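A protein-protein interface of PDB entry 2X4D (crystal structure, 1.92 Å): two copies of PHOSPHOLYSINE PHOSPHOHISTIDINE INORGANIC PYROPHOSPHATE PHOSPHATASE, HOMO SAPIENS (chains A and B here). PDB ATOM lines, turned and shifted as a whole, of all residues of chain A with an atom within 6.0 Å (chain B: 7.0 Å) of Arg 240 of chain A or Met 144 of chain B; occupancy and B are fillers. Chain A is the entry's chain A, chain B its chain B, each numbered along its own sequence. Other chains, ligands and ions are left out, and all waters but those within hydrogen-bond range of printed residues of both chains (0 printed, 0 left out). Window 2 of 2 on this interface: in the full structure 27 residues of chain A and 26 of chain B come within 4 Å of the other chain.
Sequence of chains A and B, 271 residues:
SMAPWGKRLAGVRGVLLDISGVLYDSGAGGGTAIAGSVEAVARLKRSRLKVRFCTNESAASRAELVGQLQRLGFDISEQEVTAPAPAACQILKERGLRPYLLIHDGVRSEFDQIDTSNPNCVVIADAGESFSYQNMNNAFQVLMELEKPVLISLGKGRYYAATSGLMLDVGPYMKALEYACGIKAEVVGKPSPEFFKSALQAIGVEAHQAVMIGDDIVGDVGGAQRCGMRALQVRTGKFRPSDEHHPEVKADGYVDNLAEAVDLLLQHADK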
ATOM      1  N   ARG A 158     -13.734  26.265  -8.666  1.00  0.00           N
ATOM      2  CA  ARG A 158     -12.453  26.674  -8.172  1.00  0.00           C
ATOM      3  C   ARG A 158     -11.385  25.632  -8.529  1.00  0.00           C
ATOM      4  O   ARG A 158     -10.303  25.964  -9.007  1.00  0.00           O
ATOM      5  CB  ARG A 158     -12.474  26.801  -6.666  1.00  0.00           C
ATOM      6  CG  ARG A 158     -13.263  27.956  -6.039  1.00  0.00           C
ATOM      7  CD  ARG A 158     -12.523  28.217  -4.713  1.00  0.00           C
ATOM      8  NE  ARG A 158     -13.267  27.657  -3.655  1.00  0.00           N
ATOM      9  CZ  ARG A 158     -12.841  27.389  -2.436  1.00  0.00           C
ATOM     10  NH1 ARG A 158     -11.579  27.527  -2.050  1.00  0.00           N
ATOM     11  NH2 ARG A 158     -13.766  26.908  -1.596  1.00  0.00           N
ATOM     12  N   TYR A 159     -11.704  24.380  -8.215  1.00  0.00           N
ATOM     13  CA  TYR A 159     -10.786  23.253  -8.429  1.00  0.00           C
ATOM     14  C   TYR A 159     -11.548  21.928  -8.520  1.00  0.00           C
ATOM     15  O   TYR A 159     -12.733  21.867  -8.250  1.00  0.00           O
ATOM     16  CB  TYR A 159      -9.776  23.197  -7.306  1.00  0.00           C
ATOM     17  CG  TYR A 159     -10.359  23.202  -5.905  1.00  0.00           C
ATOM     18  CD1 TYR A 159     -10.880  22.033  -5.341  1.00  0.00           C
ATOM     19  CD2 TYR A 159     -10.349  24.372  -5.121  1.00  0.00           C
ATOM     20  CE1 TYR A 159     -11.393  22.022  -4.069  1.00  0.00           C
ATOM     21  CE2 TYR A 159     -10.859  24.366  -3.811  1.00  0.00           C
ATOM     22  CZ  TYR A 159     -11.372  23.192  -3.292  1.00  0.00           C
ATOM     23  OH  TYR A 159     -11.868  23.146  -1.993  1.00  0.00           O
ATOM     24  N   LEU A 166      -5.347  18.085  -6.189  1.00  0.00           N
ATOM     25  CA  LEU A 166      -6.297  19.117  -6.541  1.00  0.00           C
ATOM     26  C   LEU A 166      -5.753  19.936  -7.692  1.00  0.00           C
ATOM     27  O   LEU A 166      -4.581  20.238  -7.744  1.00  0.00           O
ATOM     28  CB  LEU A 166      -6.645  20.016  -5.367  1.00  0.00           C
ATOM     29  CG  LEU A 166      -7.526  19.430  -4.265  1.00  0.00           C
ATOM     30  CD1 LEU A 166      -7.771  20.587  -3.237  1.00  0.00           C
ATOM     31  CD2 LEU A 166      -8.798  18.791  -4.710  1.00  0.00           C
ATOM     32  N   GLN A 233     -24.306  16.118  -0.946  1.00  0.00           N
ATOM     33  CA  GLN A 233     -22.860  16.250  -1.078  1.00  0.00           C
ATOM     34  C   GLN A 233     -22.173  14.907  -0.821  1.00  0.00           C
ATOM     35  O   GLN A 233     -22.397  14.283   0.210  1.00  0.00           O
ATOM     36  CB  GLN A 233     -22.369  17.267  -0.025  1.00  0.00           C
ATOM     37  CG  GLN A 233     -20.847  17.419   0.096  1.00  0.00           C
ATOM     38  CD  GLN A 233     -20.206  18.134  -1.093  1.00  0.00           C
ATOM     39  OE1 GLN A 233     -20.726  19.145  -1.551  1.00  0.00           O
ATOM     40  NE2 GLN A 233     -19.008  17.640  -1.542  1.00  0.00           N
ATOM     41  N   LYS A 238     -13.628  16.267  -4.904  1.00  0.00           N
ATOM     42  CA  LYS A 238     -12.968  17.469  -4.386  1.00  0.00           C
ATOM     43  C   LYS A 238     -13.332  17.811  -2.944  1.00  0.00           C
ATOM     44  O   LYS A 238     -12.750  18.766  -2.370  1.00  0.00           O
ATOM     45  CB  LYS A 238     -13.258  18.699  -5.255  1.00  0.00           C
ATOM     46  CG  LYS A 238     -14.630  19.286  -5.114  1.00  0.00           C
ATOM     47  CD  LYS A 238     -14.873  20.447  -6.073  1.00  0.00           C
ATOM     48  CE  LYS A 238     -15.348  19.983  -7.428  1.00  0.00           C
ATOM     49  NZ  LYS A 238     -15.417  21.076  -8.428  1.00  0.00           N
ATOM     50  N   PHE A 239     -14.287  17.059  -2.386  1.00  0.00           N
ATOM     51  CA  PHE A 239     -14.762  17.281  -1.015  1.00  0.00           C
ATOM     52  C   PHE A 239     -13.639  17.331   0.017  1.00  0.00           C
ATOM     53  O   PHE A 239     -12.774  16.433   0.051  1.00  0.00           O
ATOM     54  CB  PHE A 239     -15.706  16.166  -0.602  1.00  0.00           C
ATOM     55  CG  PHE A 239     -16.070  16.191   0.855  1.00  0.00           C
ATOM     56  CD1 PHE A 239     -17.205  16.898   1.287  1.00  0.00           C
ATOM     57  CD2 PHE A 239     -15.295  15.537   1.791  1.00  0.00           C
ATOM     58  CE1 PHE A 239     -17.583  16.892   2.650  1.00  0.00           C
ATOM     59  CE2 PHE A 239     -15.654  15.532   3.152  1.00  0.00           C
ATOM     60  CZ  PHE A 239     -16.798  16.227   3.584  1.00  0.00           C
ATOM     61  N   ARG A 240     -13.669  18.367   0.853  1.00  0.00           N
ATOM     62  CA  ARG A 240     -12.860  18.432   2.079  1.00  0.00           C
ATOM     63  C   ARG A 240     -13.792  18.581   3.307  1.00  0.00           C
ATOM     64  O   ARG A 240     -14.934  19.053   3.139  1.00  0.00           O
ATOM     65  CB  ARG A 240     -11.899  19.587   2.024  1.00  0.00           C
ATOM     66  CG  ARG A 240     -10.795  19.295   1.022  1.00  0.00           C
ATOM     67  CD  ARG A 240      -9.742  20.335   0.922  1.00  0.00           C
ATOM     68  NE  ARG A 240      -8.537  19.727   0.330  1.00  0.00           N
ATOM     69  CZ  ARG A 240      -7.321  20.250   0.379  1.00  0.00           C
ATOM     70  NH1 ARG A 240      -7.082  21.421   0.987  1.00  0.00           N
ATOM     71  NH2 ARG A 240      -6.325  19.576  -0.179  1.00  0.00           N
ATOM     72  N   PRO A 241     -13.361  18.069   4.467  1.00  0.00           N
ATOM     73  CA  PRO A 241     -14.243  18.119   5.635  1.00  0.00           C
ATOM     74  C   PRO A 241     -14.879  19.500   5.962  1.00  0.00           C
ATOM     75  O   PRO A 241     -16.035  19.500   6.329  1.00  0.00           O
ATOM     76  CB  PRO A 241     -13.361  17.633   6.789  1.00  0.00           C
ATOM     77  CG  PRO A 241     -12.409  16.581   6.032  1.00  0.00           C
ATOM     78  CD  PRO A 241     -12.100  17.330   4.741  1.00  0.00           C
ATOM     79  N   SER A 242     -14.199  20.621   5.740  1.00  0.00           N
ATOM     80  CA  SER A 242     -14.817  21.952   5.981  1.00  0.00           C
ATOM     81  C   SER A 242     -16.133  22.175   5.168  1.00  0.00           C
ATOM     82  O   SER A 242     -16.986  22.935   5.623  1.00  0.00           O
ATOM     83  CB  SER A 242     -13.828  23.083   5.681  1.00  0.00           C
ATOM     84  OG  SER A 242     -13.354  22.980   4.332  1.00  0.00           O
ATOM     85  N   ASP A 243     -16.278  21.471   4.030  1.00  0.00           N
ATOM     86  CA  ASP A 243     -17.453  21.536   3.129  1.00  0.00           C
ATOM     87  C   ASP A 243     -18.733  20.996   3.748  1.00  0.00           C
ATOM     88  O   ASP A 243     -19.812  21.288   3.258  1.00  0.00           O
ATOM     89  CB  ASP A 243     -17.232  20.755   1.829  1.00  0.00           C
ATOM     90  CG  ASP A 243     -16.125  21.379   0.918  1.00  0.00           C
ATOM     91  OD1 ASP A 243     -15.776  22.580   1.051  1.00  0.00           O
ATOM     92  OD2 ASP A 243     -15.691  20.633   0.027  1.00  0.00           O
ATOM     93  N   GLU A 244     -18.604  20.183   4.791  1.00  0.00           N
ATOM     94  CA  GLU A 244     -19.731  19.660   5.521  1.00  0.00           C
ATOM     95  C   GLU A 244     -20.207  20.650   6.596  1.00  0.00           C
ATOM     96  O   GLU A 244     -21.217  20.388   7.206  1.00  0.00           O
ATOM     97  CB  GLU A 244     -19.361  18.349   6.176  1.00  0.00           C
ATOM     98  CG  GLU A 244     -20.501  17.601   6.837  1.00  0.00           C
ATOM     99  CD  GLU A 244     -20.328  16.086   6.763  1.00  0.00           C
ATOM    100  OE1 GLU A 244     -19.289  15.583   6.242  1.00  0.00           O
ATOM    101  OE2 GLU A 244     -21.221  15.414   7.269  1.00  0.00           O
ATOM    102  N   ALA B 139       1.852  26.134  -7.145  1.00  0.00           N
ATOM    103  CA  ALA B 139       1.639  27.166  -6.103  1.00  0.00           C
ATOM    104  C   ALA B 139       0.316  26.888  -5.363  1.00  0.00           C
ATOM    105  O   ALA B 139       0.283  26.927  -4.136  1.00  0.00           O
ATOM    106  CB  ALA B 139       1.651  28.556  -6.694  1.00  0.00           C
ATOM    107  N   PHE B 140      -0.747  26.635  -6.134  1.00  0.00           N
ATOM    108  CA  PHE B 140      -2.053  26.243  -5.627  1.00  0.00           C
ATOM    109  C   PHE B 140      -2.018  25.043  -4.700  1.00  0.00           C
ATOM    110  O   PHE B 140      -2.594  25.045  -3.614  1.00  0.00           O
ATOM    111  CB  PHE B 140      -2.998  25.937  -6.816  1.00  0.00           C
ATOM    112  CG  PHE B 140      -4.329  25.358  -6.413  1.00  0.00           C
ATOM    113  CD1 PHE B 140      -5.226  26.095  -5.636  1.00  0.00           C
ATOM    114  CD2 PHE B 140      -4.708  24.092  -6.862  1.00  0.00           C
ATOM    115  CE1 PHE B 140      -6.447  25.567  -5.282  1.00  0.00           C
ATOM    116  CE2 PHE B 140      -5.961  23.533  -6.507  1.00  0.00           C
ATOM    117  CZ  PHE B 140      -6.810  24.257  -5.717  1.00  0.00           C
ATOM    118  N   GLN B 141      -1.323  23.997  -5.126  1.00  0.00           N
ATOM    119  CA  GLN B 141      -1.255  22.797  -4.321  1.00  0.00           C
ATOM    120  C   GLN B 141      -0.425  23.018  -3.035  1.00  0.00           C
ATOM    121  O   GLN B 141      -0.771  22.458  -1.993  1.00  0.00           O
ATOM    122  CB  GLN B 141      -0.712  21.622  -5.125  1.00  0.00           C
ATOM    123  CG  GLN B 141      -1.711  21.103  -6.171  1.00  0.00           C
ATOM    124  CD  GLN B 141      -1.223  19.842  -6.900  1.00  0.00           C
ATOM    125  OE1 GLN B 141      -0.040  19.537  -6.885  1.00  0.00           O
ATOM    126  NE2 GLN B 141      -2.147  19.102  -7.518  1.00  0.00           N
ATOM    127  N   VAL B 142       0.607  23.842  -3.087  1.00  0.00           N
ATOM    128  CA  VAL B 142       1.304  24.258  -1.846  1.00  0.00           C
ATOM    129  C   VAL B 142       0.292  24.942  -0.881  1.00  0.00           C
ATOM    130  O   VAL B 142       0.163  24.563   0.285  1.00  0.00           O
ATOM    131  CB  VAL B 142       2.499  25.181  -2.134  1.00  0.00           C
ATOM    132  CG1 VAL B 142       2.952  25.895  -0.848  1.00  0.00           C
ATOM    133  CG2 VAL B 142       3.679  24.395  -2.750  1.00  0.00           C
ATOM    134  N   LEU B 143      -0.456  25.919  -1.377  1.00  0.00           N
ATOM    135  CA  LEU B 143      -1.358  26.686  -0.504  1.00  0.00           C
ATOM    136  C   LEU B 143      -2.435  25.795   0.117  1.00  0.00           C
ATOM    137  O   LEU B 143      -2.796  25.977   1.271  1.00  0.00           O
ATOM    138  CB  LEU B 143      -1.985  27.866  -1.270  1.00  0.00           C
ATOM    139  CG  LEU B 143      -1.020  29.006  -1.585  1.00  0.00           C
ATOM    140  CD1 LEU B 143      -1.532  29.852  -2.723  1.00  0.00           C
ATOM    141  CD2 LEU B 143      -0.740  29.829  -0.320  1.00  0.00           C
ATOM    142  N   MET B 144      -2.917  24.817  -0.651  1.00  0.00           N
ATOM    143  CA  MET B 144      -4.026  23.973  -0.222  1.00  0.00           C
ATOM    144  C   MET B 144      -3.616  22.927   0.816  1.00  0.00           C
ATOM    145  O   MET B 144      -4.489  22.270   1.376  1.00  0.00           O
ATOM    146  CB  MET B 144      -4.723  23.303  -1.405  1.00  0.00           C
ATOM    147  CG  MET B 144      -5.520  24.247  -2.289  1.00  0.00           C
ATOM    148  SD  MET B 144      -6.664  25.317  -1.402  1.00  0.00           S
ATOM    149  CE  MET B 144      -8.045  24.215  -1.181  1.00  0.00           C
ATOM    150  N   GLU B 145      -2.315  22.780   1.083  1.00  0.00           N
ATOM    151  CA  GLU B 145      -1.858  21.900   2.138  1.00  0.00           C
ATOM    152  C   GLU B 145      -1.408  22.600   3.419  1.00  0.00           C
ATOM    153  O   GLU B 145      -1.204  21.958   4.422  1.00  0.00           O
ATOM    154  CB  GLU B 145      -0.751  21.012   1.601  1.00  0.00           C
ATOM    155  CG  GLU B 145      -1.214  20.150   0.438  1.00  0.00           C
ATOM    156  CD  GLU B 145      -2.548  19.400   0.692  1.00  0.00           C
ATOM    157  OE1 GLU B 145      -2.834  18.937   1.803  1.00  0.00           O
ATOM    158  OE2 GLU B 145      -3.326  19.260  -0.260  1.00  0.00           O
ATOM    159  N   LEU B 146      -1.293  23.923   3.389  1.00  0.00           N
ATOM    160  CA  LEU B 146      -0.871  24.677   4.562  1.00  0.00           C
ATOM    161  C   LEU B 146      -1.969  24.774   5.639  1.00  0.00           C
ATOM    162  O   LEU B 146      -3.133  24.997   5.333  1.00  0.00           O
ATOM    163  CB  LEU B 146      -0.397  26.057   4.124  1.00  0.00           C
ATOM    164  CG  LEU B 146       0.867  26.006   3.248  1.00  0.00           C
ATOM    165  CD1 LEU B 146       1.161  27.377   2.641  1.00  0.00           C
ATOM    166  CD2 LEU B 146       2.099  25.453   4.031  1.00  0.00           C
ATOM    167  N   GLU B 147      -1.575  24.581   6.893  1.00  0.00           N
ATOM    168  CA  GLU B 147      -2.409  24.914   8.058  1.00  0.00           C
ATOM    169  C   GLU B 147      -2.905  26.359   7.947  1.00  0.00           C
ATOM    170  O   GLU B 147      -4.121  26.591   7.928  1.00  0.00           O
ATOM    171  CB  GLU B 147      -1.609  24.768   9.364  1.00  0.00           C
ATOM    172  CG  GLU B 147      -2.491  24.351  10.544  1.00  0.00           C
ATOM    173  CD  GLU B 147      -1.834  24.477  11.868  1.00  0.00           C
ATOM    174  OE1 GLU B 147      -2.488  24.120  12.866  1.00  0.00           O
ATOM    175  OE2 GLU B 147      -0.668  24.924  11.945  1.00  0.00           O
ATOM    176  N   PRO B 149      -2.656  29.260   5.248  1.00  0.00           N
ATOM    177  CA  PRO B 149      -2.174  29.657   3.923  1.00  0.00           C
ATOM    178  C   PRO B 149      -1.969  31.168   3.778  1.00  0.00           C
ATOM    179  O   PRO B 149      -2.883  31.925   4.070  1.00  0.00           O
ATOM    180  CB  PRO B 149      -3.268  29.150   2.976  1.00  0.00           C
ATOM    181  CG  PRO B 149      -4.449  28.895   3.805  1.00  0.00           C
ATOM    182  CD  PRO B 149      -4.086  28.906   5.241  1.00  0.00           C
ATOM    183  N   LEU B 177      -5.510  32.760  -7.642  1.00  0.00           N
ATOM    184  CA  LEU B 177      -5.220  32.022  -6.412  1.00  0.00           C
ATOM    185  C   LEU B 177      -6.118  32.407  -5.232  1.00  0.00           C
ATOM    186  O   LEU B 177      -6.519  31.554  -4.472  1.00  0.00           O
ATOM    187  CB  LEU B 177      -3.766  32.143  -6.022  1.00  0.00           C
ATOM    188  CG  LEU B 177      -2.722  31.575  -6.997  1.00  0.00           C
ATOM    189  CD1 LEU B 177      -1.260  31.745  -6.413  1.00  0.00           C
ATOM    190  CD2 LEU B 177      -2.991  30.135  -7.377  1.00  0.00           C
ATOM    191  N   ALA B 180      -9.261  30.482  -6.019  1.00  0.00           N
ATOM    192  CA  ALA B 180      -8.990  29.060  -5.945  1.00  0.00           C
ATOM    193  C   ALA B 180      -8.828  28.565  -4.520  1.00  0.00           C
ATOM    194  O   ALA B 180      -9.372  27.511  -4.180  1.00  0.00           O
ATOM    195  CB  ALA B 180      -7.727  28.686  -6.750  1.00  0.00           C
ATOM    196  N   CYS B 181      -8.053  29.295  -3.714  1.00  0.00           N
ATOM    197  CA  CYS B 181      -7.781  28.909  -2.333  1.00  0.00           C
ATOM    198  C   CYS B 181      -8.740  29.457  -1.292  1.00  0.00           C
ATOM    199  O   CYS B 181      -8.749  28.976  -0.170  1.00  0.00           O
ATOM    200  CB  CYS B 181      -6.384  29.331  -1.940  1.00  0.00           C
ATOM    201  SG  CYS B 181      -5.167  28.596  -3.041  1.00  0.00           S
ATOM    202  N   GLY B 182      -9.545  30.449  -1.649  1.00  0.00           N
ATOM    203  CA  GLY B 182     -10.394  31.143  -0.668  1.00  0.00           C
ATOM    204  C   GLY B 182      -9.642  31.941   0.384  1.00  0.00           C
ATOM    205  O   GLY B 182     -10.017  31.917   1.571  1.00  0.00           O
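Of chain B, only Met 144 and Glu 145 come within 4 Å of Arg 240 of chain A.
Printed residues of chain A within 4 Å of Gln 141 of chain B: Leu 166.
Val 142 of chain B touches none of the printed residues of chain A.
Met 144 of chain B touches just these residues of chain A: Tyr 159 (3.9 Å) and Arg 240 (2.8 Å).
Of the printed residues of chain A, Glu 145 of chain B touches Arg 240.
Printed residues of chain A within 4 Å of Ala 180 of chain B: Arg 158 (3.1 Å) and Tyr 159 (3.4 Å).
Printed residues of chain A within 4 Å of Cys 181 of chain B: Arg 158 (3.5 Å).
The nearest residue of chain A that does not touch Met 144 of chain B is Leu 166 of chain A (4.2 Å).
The nearest printed residue of chain B that does not touch Tyr 159 of chain A is Cys 181 of chain B (5.6 Å).
No position is printed for both chains.
Of the 10 pairs that touch across the chains among the printed residues, none has its exchanged pair printed and touching as well.
Among the printed residues, merely in contact across the chains: Tyr 159 of chain A with Ala 180 of chain B (3.4 Å), Arg 158 of chain A with Cys 181 of chain B (3.5 Å), Tyr 159 of chain A with Phe 140 of chain B (3.5 Å), Arg 158 of chain A with Gly 182 of chain B (3.6 Å), Leu 166 of chain A with Phe 140 of chain B (3.8 Å) and Tyr 159 of chain A with Met 144 of chain B (3.9 Å).
The side-chain amino group (NZ) of Lys 238 of chain A sits at hydrogen-bond distance from the backbone carbonyl oxygen (O) of Tyr 159 of chain A, 2.8 Å away.
N of Arg 240 of chain A lies within hydrogen-bond range of OD2 of Asp 243 of chain A, at 3.1 Å.
SG of Cys 181 of chain B lies close to O of Leu 177 of chain B, 3.6 Å away.
The guanidinium group (NH1) of Arg 158 of chain A sits at hydrogen-bond distance from the backbone carbonyl oxygen (O) of Ala 180 of chain B.
The side-chain amide nitrogen (NE2) of Gln 141 of chain B sits at hydrogen-bond distance from the backbone carbonyl oxygen (O) of Leu 166 of chain A.
NH1 of Arg 240 of chain A is in hydrogen-bond range of O of Met 144 of chain B (2.8 Å).
The guanidinium group (NH2) of Arg 240 of chain A is in salt-bridge range of the side-chain carboxylate (OE2) of Glu 145 of chain B (3.0 Å).
Of the 14 printed residues of chain B, 7 touch a printed residue of chain A.
Among the printed residues, 10 pairs touch across the chains.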
